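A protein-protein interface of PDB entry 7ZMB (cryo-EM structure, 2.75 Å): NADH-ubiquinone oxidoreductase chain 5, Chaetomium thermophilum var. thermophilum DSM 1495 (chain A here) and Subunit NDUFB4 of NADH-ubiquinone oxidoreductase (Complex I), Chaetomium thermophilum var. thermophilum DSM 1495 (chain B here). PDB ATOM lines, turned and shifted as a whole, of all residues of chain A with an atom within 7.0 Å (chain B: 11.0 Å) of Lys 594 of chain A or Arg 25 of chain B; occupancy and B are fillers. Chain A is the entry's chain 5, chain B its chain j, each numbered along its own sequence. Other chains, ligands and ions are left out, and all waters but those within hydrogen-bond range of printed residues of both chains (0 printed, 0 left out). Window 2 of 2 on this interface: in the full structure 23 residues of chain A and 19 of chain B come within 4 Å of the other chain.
Of the 14 printed residues of chain A, 8 touch a printed residue of chain B.
Printed residues of chain A that touch a printed residue of chain B: Leu 588, Gln 591, Lys 594, Ile 595, Leu 596, Lys 598, Gly 599 and Ser 600.
Of the 22 printed residues of chain B, 9 touch a printed residue of chain A.
Printed residues of chain B that touch a printed residue of chain A: Ile 22, Arg 25, Tyr 26, Phe 29, Trp 31, Thr 35, Val 38, Ser 39 and Tyr 42.
Hydrophobic or aromatic side chains of chain B within 4 Å of the printed part of chain A: Phe 29, Trp 31, Val 38 and Tyr 42.
Of chain B, only Arg 25 (3.4 Å) comes within 4 Å of Lys 594 of chain A.
No residue of chain B comes within 4 Å of Gly 590 of chain A.
No residue of chain B comes within 4 Å of Thr 593 of chain A.
Of the printed residues of chain B, Ile 595 of chain A touches Phe 29 (3.5 Å), Thr 35 (3.6 Å) and Val 38 (3.7 Å).
Asp 597 of chain A touches none of the printed residues of chain B.
Of the printed residues of chain B, Gly 599 of chain A touches Phe 29.
Of the printed residues of chain B, Leu 596 of chain A touches Ser 39 and Tyr 42.
Of the printed residues of chain A, Ser 39 of chain B touches Leu 596 (3.7 Å) and Ser 600 (2.7 Å).
Of the printed residues of chain A, Thr 35 of chain B touches Ile 595.
Gly 589 of chain A touches none of the printed residues of chain B.
Asn 24 of chain B touches none of the printed residues of chain A.
The nearest printed residue of chain B that does not touch Leu 596 of chain A is Val 38 of chain B (4.3 Å).
Tyr 42 of chain B touches Leu 588 of chain A (OH to CD1, 3.2 Å).
Gln 591 of chain A touches Tyr 42 of chain B (CB to CE2, 3.9 Å).
O of Ile 595 of chain A touches CE1 of Phe 29 of chain B (3.5 Å).
CG2 of Thr 35 of chain B touches CG2 of Ile 595 of chain A, at 3.6 Å.
Ile 595 of chain A touches Val 38 of chain B.
Leu 596 of chain A touches Ser 39 of chain B.
Lys 598 of chain A touches Ile 22 of chain B (CD to O, 3.8 Å).
Lys 598 of chain A touches Arg 25 of chain B.
Gly 599 of chain A touches Phe 29 of chain B (C to CG, 3.6 Å).
Trp 31 of chain B touches Ser 600 of chain A (CH2 to CB, 3.4 Å).
The side-chain sulfur of Met 21 of chain B is in hydrogen-bond range of the guanidinium group of Arg 25 of chain B, at 3.2 Å.
The side-chain hydroxyl (OH) of Tyr 26 of chain B sits at hydrogen-bond distance from the side-chain amino group (NZ) of Lys 27 of chain B (3.3 Å).
The side-chain hydroxyl of Ser 39 of chain B lies within hydrogen-bond range of the backbone carbonyl oxygen of Thr 35 of chain B (3.3 Å).
N of Ser 600 of chain A sits at hydrogen-bond distance from O of Ile 595 of chain A.
The side-chain hydroxyl (OG) of Ser 39 of chain B lies within hydrogen-bond range of the side-chain hydroxyl (OG) of Ser 600 of chain A, 2.7 Å away.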
ATOM      1  N   ASN A 587       7.193  20.103  -2.361  1.00  0.00           N
ATOM      2  CA  ASN A 587       7.410  21.219  -1.448  1.00  0.00           C
ATOM      3  C   ASN A 587       6.759  22.517  -1.905  1.00  0.00           C
ATOM      4  O   ASN A 587       6.329  23.304  -1.061  1.00  0.00           O
ATOM      5  CB  ASN A 587       8.906  21.459  -1.215  1.00  0.00           C
ATOM      6  CG  ASN A 587       9.582  20.298  -0.529  1.00  0.00           C
ATOM      7  OD1 ASN A 587      10.444  19.638  -1.096  1.00  0.00           O
ATOM      8  ND2 ASN A 587       9.185  20.035   0.708  1.00  0.00           N
ATOM      9  N   LEU A 588       6.691  22.781  -3.211  1.00  0.00           N
ATOM     10  CA  LEU A 588       5.853  23.883  -3.676  1.00  0.00           C
ATOM     11  C   LEU A 588       4.408  23.688  -3.250  1.00  0.00           C
ATOM     12  O   LEU A 588       3.755  24.635  -2.799  1.00  0.00           O
ATOM     13  CB  LEU A 588       5.953  24.052  -5.192  1.00  0.00           C
ATOM     14  CG  LEU A 588       7.102  24.869  -5.772  1.00  0.00           C
ATOM     15  CD1 LEU A 588       6.951  26.291  -5.310  1.00  0.00           C
ATOM     16  CD2 LEU A 588       8.438  24.366  -5.323  1.00  0.00           C
ATOM     17  N   GLY A 589       3.895  22.466  -3.365  1.00  0.00           N
ATOM     18  CA  GLY A 589       2.598  22.173  -2.793  1.00  0.00           C
ATOM     19  C   GLY A 589       2.559  22.411  -1.301  1.00  0.00           C
ATOM     20  O   GLY A 589       1.545  22.869  -0.770  1.00  0.00           O
ATOM     21  N   GLY A 590       3.656  22.107  -0.608  1.00  0.00           N
ATOM     22  CA  GLY A 590       3.716  22.356   0.821  1.00  0.00           C
ATOM     23  C   GLY A 590       3.727  23.830   1.170  1.00  0.00           C
ATOM     24  O   GLY A 590       3.087  24.251   2.135  1.00  0.00           O
ATOM     25  N   GLN A 591       4.473  24.635   0.408  1.00  0.00           N
ATOM     26  CA  GLN A 591       4.489  26.075   0.646  1.00  0.00           C
ATOM     27  C   GLN A 591       3.125  26.701   0.377  1.00  0.00           C
ATOM     28  O   GLN A 591       2.663  27.553   1.142  1.00  0.00           O
ATOM     29  CB  GLN A 591       5.554  26.744  -0.219  1.00  0.00           C
ATOM     30  CG  GLN A 591       6.975  26.365   0.125  1.00  0.00           C
ATOM     31  CD  GLN A 591       7.517  27.145   1.306  1.00  0.00           C
ATOM     32  OE1 GLN A 591       7.683  26.602   2.398  1.00  0.00           O
ATOM     33  NE2 GLN A 591       7.800  28.425   1.091  1.00  0.00           N
ATOM     34  N   ILE A 592       2.464  26.286  -0.707  1.00  0.00           N
ATOM     35  CA  ILE A 592       1.195  26.896  -1.094  1.00  0.00           C
ATOM     36  C   ILE A 592       0.111  26.574  -0.079  1.00  0.00           C
ATOM     37  O   ILE A 592      -0.696  27.437   0.279  1.00  0.00           O
ATOM     38  CB  ILE A 592       0.788  26.436  -2.505  1.00  0.00           C
ATOM     39  CG1 ILE A 592       1.725  27.006  -3.553  1.00  0.00           C
ATOM     40  CG2 ILE A 592      -0.628  26.867  -2.830  1.00  0.00           C
ATOM     41  CD1 ILE A 592       1.666  26.248  -4.845  1.00  0.00           C
ATOM     42  N   THR A 593       0.064  25.337   0.400  1.00  0.00           N
ATOM     43  CA  THR A 593      -1.053  24.907   1.227  1.00  0.00           C
ATOM     44  C   THR A 593      -0.854  25.195   2.708  1.00  0.00           C
ATOM     45  O   THR A 593      -1.781  24.975   3.491  1.00  0.00           O
ATOM     46  CB  THR A 593      -1.317  23.411   1.020  1.00  0.00           C
ATOM     47  OG1 THR A 593      -2.622  23.088   1.505  1.00  0.00           O
ATOM     48  CG2 THR A 593      -0.285  22.570   1.750  1.00  0.00           C
ATOM     49  N   LYS A 594       0.321  25.678   3.111  1.00  0.00           N
ATOM     50  CA  LYS A 594       0.582  26.070   4.492  1.00  0.00           C
ATOM     51  C   LYS A 594       0.765  27.570   4.647  1.00  0.00           C
ATOM     52  O   LYS A 594       0.078  28.196   5.452  1.00  0.00           O
ATOM     53  CB  LYS A 594       1.816  25.341   5.035  1.00  0.00           C
ATOM     54  CG  LYS A 594       1.734  23.836   4.955  1.00  0.00           C
ATOM     55  CD  LYS A 594       2.846  23.182   5.758  1.00  0.00           C
ATOM     56  CE  LYS A 594       3.795  22.411   4.869  1.00  0.00           C
ATOM     57  NZ  LYS A 594       4.917  21.831   5.633  1.00  0.00           N
ATOM     58  N   ILE A 595       1.690  28.161   3.893  1.00  0.00           N
ATOM     59  CA  ILE A 595       1.890  29.604   3.954  1.00  0.00           C
ATOM     60  C   ILE A 595       0.729  30.348   3.295  1.00  0.00           C
ATOM     61  O   ILE A 595       0.284  31.382   3.796  1.00  0.00           O
ATOM     62  CB  ILE A 595       3.244  29.994   3.325  1.00  0.00           C
ATOM     63  CG1 ILE A 595       4.412  29.397   4.109  1.00  0.00           C
ATOM     64  CG2 ILE A 595       3.391  31.499   3.244  1.00  0.00           C
ATOM     65  CD1 ILE A 595       4.892  28.070   3.600  1.00  0.00           C
ATOM     66  N   LEU A 596       0.224  29.858   2.164  1.00  0.00           N
ATOM     67  CA  LEU A 596      -0.770  30.635   1.412  1.00  0.00           C
ATOM     68  C   LEU A 596      -2.201  30.276   1.801  1.00  0.00           C
ATOM     69  O   LEU A 596      -2.900  31.091   2.404  1.00  0.00           O
ATOM     70  CB  LEU A 596      -0.561  30.457  -0.093  1.00  0.00           C
ATOM     71  CG  LEU A 596       0.795  30.878  -0.648  1.00  0.00           C
ATOM     72  CD1 LEU A 596       0.736  30.881  -2.151  1.00  0.00           C
ATOM     73  CD2 LEU A 596       1.184  32.241  -0.121  1.00  0.00           C
ATOM     74  N   ASP A 597      -2.625  29.047   1.515  1.00  0.00           N
ATOM     75  CA  ASP A 597      -4.033  28.695   1.658  1.00  0.00           C
ATOM     76  C   ASP A 597      -4.487  28.778   3.103  1.00  0.00           C
ATOM     77  O   ASP A 597      -5.297  29.639   3.459  1.00  0.00           O
ATOM     78  CB  ASP A 597      -4.314  27.290   1.136  1.00  0.00           C
ATOM     79  CG  ASP A 597      -4.222  27.194  -0.361  1.00  0.00           C
ATOM     80  OD1 ASP A 597      -3.785  28.167  -0.996  1.00  0.00           O
ATOM     81  OD2 ASP A 597      -4.629  26.153  -0.908  1.00  0.00           O
ATOM     82  N   LYS A 598      -3.956  27.902   3.949  1.00  0.00           N
ATOM     83  CA  LYS A 598      -4.226  27.966   5.380  1.00  0.00           C
ATOM     84  C   LYS A 598      -3.248  28.916   6.055  1.00  0.00           C
ATOM     85  O   LYS A 598      -2.659  28.622   7.090  1.00  0.00           O
ATOM     86  CB  LYS A 598      -4.136  26.569   5.976  1.00  0.00           C
ATOM     87  CG  LYS A 598      -5.252  25.633   5.555  1.00  0.00           C
ATOM     88  CD  LYS A 598      -4.757  24.203   5.453  1.00  0.00           C
ATOM     89  CE  LYS A 598      -5.897  23.249   5.184  1.00  0.00           C
ATOM     90  NZ  LYS A 598      -6.980  23.882   4.385  1.00  0.00           N
ATOM     91  N   GLY A 599      -3.094  30.087   5.444  1.00  0.00           N
ATOM     92  CA  GLY A 599      -2.068  31.047   5.792  1.00  0.00           C
ATOM     93  C   GLY A 599      -2.463  32.487   5.552  1.00  0.00           C
ATOM     94  O   GLY A 599      -3.471  32.978   6.064  1.00  0.00           O
ATOM     95  N   SER A 600      -1.622  33.174   4.781  1.00  0.00           N
ATOM     96  CA  SER A 600      -1.852  34.572   4.430  1.00  0.00           C
ATOM     97  C   SER A 600      -3.183  34.786   3.719  1.00  0.00           C
ATOM     98  O   SER A 600      -3.833  35.819   3.921  1.00  0.00           O
ATOM     99  CB  SER A 600      -0.712  35.062   3.554  1.00  0.00           C
ATOM    100  OG  SER A 600      -0.539  34.202   2.452  1.00  0.00           O
ATOM    101  N   ARG B  17      -4.273  14.158  16.315  1.00  0.00           N
ATOM    102  CA  ARG B  17      -3.812  15.503  16.634  1.00  0.00           C
ATOM    103  C   ARG B  17      -3.150  16.178  15.444  1.00  0.00           C
ATOM    104  O   ARG B  17      -3.201  17.406  15.334  1.00  0.00           O
ATOM    105  CB  ARG B  17      -2.867  15.476  17.838  1.00  0.00           C
ATOM    106  CG  ARG B  17      -1.461  14.994  17.557  1.00  0.00           C
ATOM    107  CD  ARG B  17      -0.642  14.964  18.833  1.00  0.00           C
ATOM    108  NE  ARG B  17      -1.218  14.058  19.821  1.00  0.00           N
ATOM    109  CZ  ARG B  17      -0.814  13.978  21.085  1.00  0.00           C
ATOM    110  NH1 ARG B  17      -1.396  13.126  21.916  1.00  0.00           N
ATOM    111  NH2 ARG B  17       0.172  14.752  21.516  1.00  0.00           N
ATOM    112  N   LEU B  18      -2.539  15.409  14.544  1.00  0.00           N
ATOM    113  CA  LEU B  18      -1.990  15.998  13.327  1.00  0.00           C
ATOM    114  C   LEU B  18      -3.089  16.588  12.451  1.00  0.00           C
ATOM    115  O   LEU B  18      -2.896  17.633  11.823  1.00  0.00           O
ATOM    116  CB  LEU B  18      -1.180  14.956  12.563  1.00  0.00           C
ATOM    117  CG  LEU B  18      -0.479  15.411  11.286  1.00  0.00           C
ATOM    118  CD1 LEU B  18       0.536  16.469  11.573  1.00  0.00           C
ATOM    119  CD2 LEU B  18       0.196  14.219  10.668  1.00  0.00           C
ATOM    120  N   GLY B  19      -4.246  15.929  12.391  1.00  0.00           N
ATOM    121  CA  GLY B  19      -5.380  16.495  11.686  1.00  0.00           C
ATOM    122  C   GLY B  19      -5.900  17.768  12.319  1.00  0.00           C
ATOM    123  O   GLY B  19      -6.356  18.673  11.615  1.00  0.00           O
ATOM    124  N   SER B  20      -5.850  17.857  13.649  1.00  0.00           N
ATOM    125  CA  SER B  20      -6.296  19.072  14.322  1.00  0.00           C
ATOM    126  C   SER B  20      -5.433  20.265  13.946  1.00  0.00           C
ATOM    127  O   SER B  20      -5.951  21.357  13.694  1.00  0.00           O
ATOM    128  CB  SER B  20      -6.286  18.871  15.833  1.00  0.00           C
ATOM    129  OG  SER B  20      -6.684  20.054  16.498  1.00  0.00           O
ATOM    130  N   MET B  21      -4.114  20.080  13.907  1.00  0.00           N
ATOM    131  CA  MET B  21      -3.223  21.190  13.594  1.00  0.00           C
ATOM    132  C   MET B  21      -3.365  21.619  12.139  1.00  0.00           C
ATOM    133  O   MET B  21      -3.380  22.817  11.837  1.00  0.00           O
ATOM    134  CB  MET B  21      -1.776  20.805  13.911  1.00  0.00           C
ATOM    135  CG  MET B  21      -0.765  21.890  13.604  1.00  0.00           C
ATOM    136  SD  MET B  21       0.115  21.646  12.051  1.00  0.00           S
ATOM    137  CE  MET B  21       0.652  19.955  12.251  1.00  0.00           C
ATOM    138  N   ILE B  22      -3.461  20.658  11.219  1.00  0.00           N
ATOM    139  CA  ILE B  22      -3.664  21.011   9.817  1.00  0.00           C
ATOM    140  C   ILE B  22      -4.979  21.758   9.655  1.00  0.00           C
ATOM    141  O   ILE B  22      -5.074  22.729   8.895  1.00  0.00           O
ATOM    142  CB  ILE B  22      -3.619  19.756   8.924  1.00  0.00           C
ATOM    143  CG1 ILE B  22      -2.285  19.031   9.055  1.00  0.00           C
ATOM    144  CG2 ILE B  22      -3.824  20.134   7.480  1.00  0.00           C
ATOM    145  CD1 ILE B  22      -1.121  19.915   9.012  1.00  0.00           C
ATOM    146  N   SER B  23      -6.010  21.317  10.372  1.00  0.00           N
ATOM    147  CA  SER B  23      -7.295  22.001  10.347  1.00  0.00           C
ATOM    148  C   SER B  23      -7.174  23.421  10.872  1.00  0.00           C
ATOM    149  O   SER B  23      -7.707  24.361  10.277  1.00  0.00           O
ATOM    150  CB  SER B  23      -8.308  21.218  11.176  1.00  0.00           C
ATOM    151  OG  SER B  23      -9.555  21.872  11.202  1.00  0.00           O
ATOM    152  N   ASN B  24      -6.464  23.597  11.984  1.00  0.00           N
ATOM    153  CA  ASN B  24      -6.447  24.851  12.715  1.00  0.00           C
ATOM    154  C   ASN B  24      -5.212  25.695  12.442  1.00  0.00           C
ATOM    155  O   ASN B  24      -5.041  26.733  13.084  1.00  0.00           O
ATOM    156  CB  ASN B  24      -6.559  24.582  14.212  1.00  0.00           C
ATOM    157  CG  ASN B  24      -7.801  23.800  14.575  1.00  0.00           C
ATOM    158  OD1 ASN B  24      -7.742  22.861  15.359  1.00  0.00           O
ATOM    159  ND2 ASN B  24      -8.933  24.191  14.011  1.00  0.00           N
ATOM    160  N   ARG B  25      -4.349  25.284  11.505  1.00  0.00           N
ATOM    161  CA  ARG B  25      -3.155  26.069  11.212  1.00  0.00           C
ATOM    162  C   ARG B  25      -3.470  27.501  10.793  1.00  0.00           C
ATOM    163  O   ARG B  25      -2.643  28.391  11.016  1.00  0.00           O
ATOM    164  CB  ARG B  25      -2.296  25.382  10.135  1.00  0.00           C
ATOM    165  CG  ARG B  25      -1.004  26.146   9.889  1.00  0.00           C
ATOM    166  CD  ARG B  25      -0.009  25.596   8.879  1.00  0.00           C
ATOM    167  NE  ARG B  25       0.590  24.323   9.246  1.00  0.00           N
ATOM    168  CZ  ARG B  25       0.399  23.171   8.621  1.00  0.00           C
ATOM    169  NH1 ARG B  25      -0.392  23.085   7.560  1.00  0.00           N
ATOM    170  NH2 ARG B  25       1.035  22.100   9.062  1.00  0.00           N
ATOM    171  N   TYR B  26      -4.645  27.757  10.217  1.00  0.00           N
ATOM    172  CA  TYR B  26      -4.919  29.096   9.704  1.00  0.00           C
ATOM    173  C   TYR B  26      -4.911  30.148  10.805  1.00  0.00           C
ATOM    174  O   TYR B  26      -4.700  31.330  10.517  1.00  0.00           O
ATOM    175  CB  TYR B  26      -6.261  29.121   8.960  1.00  0.00           C
ATOM    176  CG  TYR B  26      -7.471  29.067   9.863  1.00  0.00           C
ATOM    177  CD1 TYR B  26      -7.925  27.861  10.380  1.00  0.00           C
ATOM    178  CD2 TYR B  26      -8.137  30.220  10.221  1.00  0.00           C
ATOM    179  CE1 TYR B  26      -9.012  27.811  11.205  1.00  0.00           C
ATOM    180  CE2 TYR B  26      -9.226  30.177  11.047  1.00  0.00           C
ATOM    181  CZ  TYR B  26      -9.661  28.975  11.537  1.00  0.00           C
ATOM    182  OH  TYR B  26     -10.755  28.934  12.367  1.00  0.00           O
ATOM    183  N   LYS B  27      -5.114  29.744  12.056  1.00  0.00           N
ATOM    184  CA  LYS B  27      -5.272  30.679  13.160  1.00  0.00           C
ATOM    185  C   LYS B  27      -3.955  31.238  13.671  1.00  0.00           C
ATOM    186  O   LYS B  27      -3.969  32.204  14.435  1.00  0.00           O
ATOM    187  CB  LYS B  27      -6.004  29.995  14.315  1.00  0.00           C
ATOM    188  CG  LYS B  27      -7.508  30.001  14.192  1.00  0.00           C
ATOM    189  CD  LYS B  27      -8.162  29.522  15.472  1.00  0.00           C
ATOM    190  CE  LYS B  27      -8.106  28.007  15.588  1.00  0.00           C
ATOM    191  NZ  LYS B  27      -8.913  27.328  14.536  1.00  0.00           N
ATOM    192  N   TYR B  28      -2.824  30.660  13.278  1.00  0.00           N
ATOM    193  CA  TYR B  28      -1.536  31.017  13.856  1.00  0.00           C
ATOM    194  C   TYR B  28      -0.594  31.656  12.856  1.00  0.00           C
ATOM    195  O   TYR B  28       0.557  31.935  13.196  1.00  0.00           O
ATOM    196  CB  TYR B  28      -0.879  29.781  14.460  1.00  0.00           C
ATOM    197  CG  TYR B  28      -1.758  29.091  15.465  1.00  0.00           C
ATOM    198  CD1 TYR B  28      -1.825  29.535  16.774  1.00  0.00           C
ATOM    199  CD2 TYR B  28      -2.538  28.013  15.101  1.00  0.00           C
ATOM    200  CE1 TYR B  28      -2.625  28.913  17.695  1.00  0.00           C
ATOM    201  CE2 TYR B  28      -3.345  27.385  16.022  1.00  0.00           C
ATOM    202  CZ  TYR B  28      -3.385  27.842  17.315  1.00  0.00           C
ATOM    203  OH  TYR B  28      -4.192  27.215  18.229  1.00  0.00           O
ATOM    204  N   PHE B  29      -1.054  31.900  11.638  1.00  0.00           N
ATOM    205  CA  PHE B  29      -0.236  32.578  10.650  1.00  0.00           C
ATOM    206  C   PHE B  29       0.112  33.983  11.111  1.00  0.00           C
ATOM    207  O   PHE B  29      -0.739  34.708  11.627  1.00  0.00           O
ATOM    208  CB  PHE B  29      -0.979  32.639   9.326  1.00  0.00           C
ATOM    209  CG  PHE B  29      -0.227  33.336   8.264  1.00  0.00           C
ATOM    210  CD1 PHE B  29       0.714  32.660   7.529  1.00  0.00           C
ATOM    211  CD2 PHE B  29      -0.426  34.682   8.023  1.00  0.00           C
ATOM    212  CE1 PHE B  29       1.404  33.293   6.568  1.00  0.00           C
ATOM    213  CE2 PHE B  29       0.291  35.324   7.059  1.00  0.00           C
ATOM    214  CZ  PHE B  29       1.206  34.628   6.330  1.00  0.00           C
ATOM    215  N   ARG B  30       1.363  34.378  10.906  1.00  0.00           N
ATOM    216  CA  ARG B  30       1.798  35.739  11.173  1.00  0.00           C
ATOM    217  C   ARG B  30       2.593  36.272   9.993  1.00  0.00           C
ATOM    218  O   ARG B  30       3.042  35.526   9.126  1.00  0.00           O
ATOM    219  CB  ARG B  30       2.647  35.840  12.443  1.00  0.00           C
ATOM    220  CG  ARG B  30       1.939  35.436  13.700  1.00  0.00           C
ATOM    221  CD  ARG B  30       2.936  34.997  14.731  1.00  0.00           C
ATOM    222  NE  ARG B  30       3.865  34.006  14.199  1.00  0.00           N
ATOM    223  CZ  ARG B  30       5.154  33.955  14.504  1.00  0.00           C
ATOM    224  NH1 ARG B  30       5.662  34.848  15.332  1.00  0.00           N
ATOM    225  NH2 ARG B  30       5.932  33.019  13.981  1.00  0.00           N
ATOM    226  N   TRP B  31       2.762  37.584   9.981  1.00  0.00           N
ATOM    227  CA  TRP B  31       3.536  38.254   8.949  1.00  0.00           C
ATOM    228  C   TRP B  31       4.997  38.328   9.369  1.00  0.00           C
ATOM    229  O   TRP B  31       5.314  38.858  10.438  1.00  0.00           O
ATOM    230  CB  TRP B  31       2.975  39.650   8.707  1.00  0.00           C
ATOM    231  CG  TRP B  31       1.737  39.696   7.887  1.00  0.00           C
ATOM    232  CD1 TRP B  31       0.606  40.395   8.169  1.00  0.00           C
ATOM    233  CD2 TRP B  31       1.512  39.064   6.624  1.00  0.00           C
ATOM    234  NE1 TRP B  31      -0.317  40.226   7.172  1.00  0.00           N
ATOM    235  CE2 TRP B  31       0.216  39.413   6.210  1.00  0.00           C
ATOM    236  CE3 TRP B  31       2.280  38.236   5.802  1.00  0.00           C
ATOM    237  CZ2 TRP B  31      -0.330  38.964   5.023  1.00  0.00           C
ATOM    238  CZ3 TRP B  31       1.732  37.790   4.618  1.00  0.00           C
ATOM    239  CH2 TRP B  31       0.443  38.158   4.238  1.00  0.00           C
ATOM    240  N   ARG B  34      10.279  36.456   6.094  1.00  0.00           N
ATOM    241  CA  ARG B  34      10.169  35.308   5.202  1.00  0.00           C
ATOM    242  C   ARG B  34       8.783  35.218   4.587  1.00  0.00           C
ATOM    243  O   ARG B  34       8.634  35.141   3.361  1.00  0.00           O
ATOM    244  CB  ARG B  34      10.478  34.022   5.964  1.00  0.00           C
ATOM    245  CG  ARG B  34      10.434  32.774   5.105  1.00  0.00           C
ATOM    246  CD  ARG B  34      10.824  31.539   5.902  1.00  0.00           C
ATOM    247  NE  ARG B  34      10.691  30.315   5.118  1.00  0.00           N
ATOM    248  CZ  ARG B  34      11.640  29.834   4.321  1.00  0.00           C
ATOM    249  NH1 ARG B  34      12.795  30.473   4.200  1.00  0.00           N
ATOM    250  NH2 ARG B  34      11.435  28.712   3.644  1.00  0.00           N
ATOM    251  N   THR B  35       7.754  35.255   5.426  1.00  0.00           N
ATOM    252  CA  THR B  35       6.445  34.788   5.005  1.00  0.00           C
ATOM    253  C   THR B  35       5.775  35.771   4.054  1.00  0.00           C
ATOM    254  O   THR B  35       5.029  35.355   3.161  1.00  0.00           O
ATOM    255  CB  THR B  35       5.582  34.533   6.235  1.00  0.00           C
ATOM    256  OG1 THR B  35       6.355  33.823   7.206  1.00  0.00           O
ATOM    257  CG2 THR B  35       4.485  33.643   5.858  1.00  0.00           C
ATOM    258  N   ALA B  36       6.026  37.067   4.220  1.00  0.00           N
ATOM    259  CA  ALA B  36       5.552  38.024   3.232  1.00  0.00           C
ATOM    260  C   ALA B  36       6.259  37.838   1.894  1.00  0.00           C
ATOM    261  O   ALA B  36       5.646  38.034   0.841  1.00  0.00           O
ATOM    262  CB  ALA B  36       5.736  39.448   3.748  1.00  0.00           C
ATOM    263  N   VAL B  38       7.274  34.943   0.667  1.00  0.00           N
ATOM    264  CA  VAL B  38       6.613  33.805   0.039  1.00  0.00           C
ATOM    265  C   VAL B  38       5.244  34.210  -0.492  1.00  0.00           C
ATOM    266  O   VAL B  38       4.889  33.905  -1.636  1.00  0.00           O
ATOM    267  CB  VAL B  38       6.522  32.627   1.023  1.00  0.00           C
ATOM    268  CG1 VAL B  38       5.741  31.485   0.412  1.00  0.00           C
ATOM    269  CG2 VAL B  38       7.911  32.161   1.393  1.00  0.00           C
ATOM    270  N   SER B  39       4.459  34.914   0.326  1.00  0.00           N
ATOM    271  CA  SER B  39       3.162  35.393  -0.137  1.00  0.00           C
ATOM    272  C   SER B  39       3.315  36.350  -1.304  1.00  0.00           C
ATOM    273  O   SER B  39       2.473  36.378  -2.205  1.00  0.00           O
ATOM    274  CB  SER B  39       2.399  36.069   1.004  1.00  0.00           C
ATOM    275  OG  SER B  39       2.000  35.131   1.983  1.00  0.00           O
ATOM    276  N   TYR B  42       4.371  34.252  -4.743  1.00  0.00           N
ATOM    277  CA  TYR B  42       3.396  33.349  -5.333  1.00  0.00           C
ATOM    278  C   TYR B  42       2.066  34.021  -5.650  1.00  0.00           C
ATOM    279  O   TYR B  42       1.334  33.523  -6.513  1.00  0.00           O
ATOM    280  CB  TYR B  42       3.154  32.148  -4.410  1.00  0.00           C
ATOM    281  CG  TYR B  42       4.361  31.254  -4.151  1.00  0.00           C
ATOM    282  CD1 TYR B  42       5.584  31.498  -4.750  1.00  0.00           C
ATOM    283  CD2 TYR B  42       4.266  30.172  -3.293  1.00  0.00           C
ATOM    284  CE1 TYR B  42       6.672  30.696  -4.507  1.00  0.00           C
ATOM    285  CE2 TYR B  42       5.343  29.364  -3.041  1.00  0.00           C
ATOM    286  CZ  TYR B  42       6.548  29.627  -3.650  1.00  0.00           C
ATOM    287  OH  TYR B  42       7.633  28.819  -3.404  1.00  0.00           O
ATOM    288  N   VAL B  43       1.733  35.129  -4.996  1.00  0.00           N
ATOM    289  CA  VAL B  43       0.476  35.823  -5.249  1.00  0.00           C
ATOM    290  C   VAL B  43       0.655  36.971  -6.230  1.00  0.00           C
ATOM    291  O   VAL B  43      -0.219  37.234  -7.054  1.00  0.00           O
ATOM    292  CB  VAL B  43      -0.146  36.321  -3.926  1.00  0.00           C
ATOM    293  CG1 VAL B  43      -1.319  37.237  -4.191  1.00  0.00           C
ATOM    294  CG2 VAL B  43      -0.568  35.149  -3.064  1.00  0.00           C
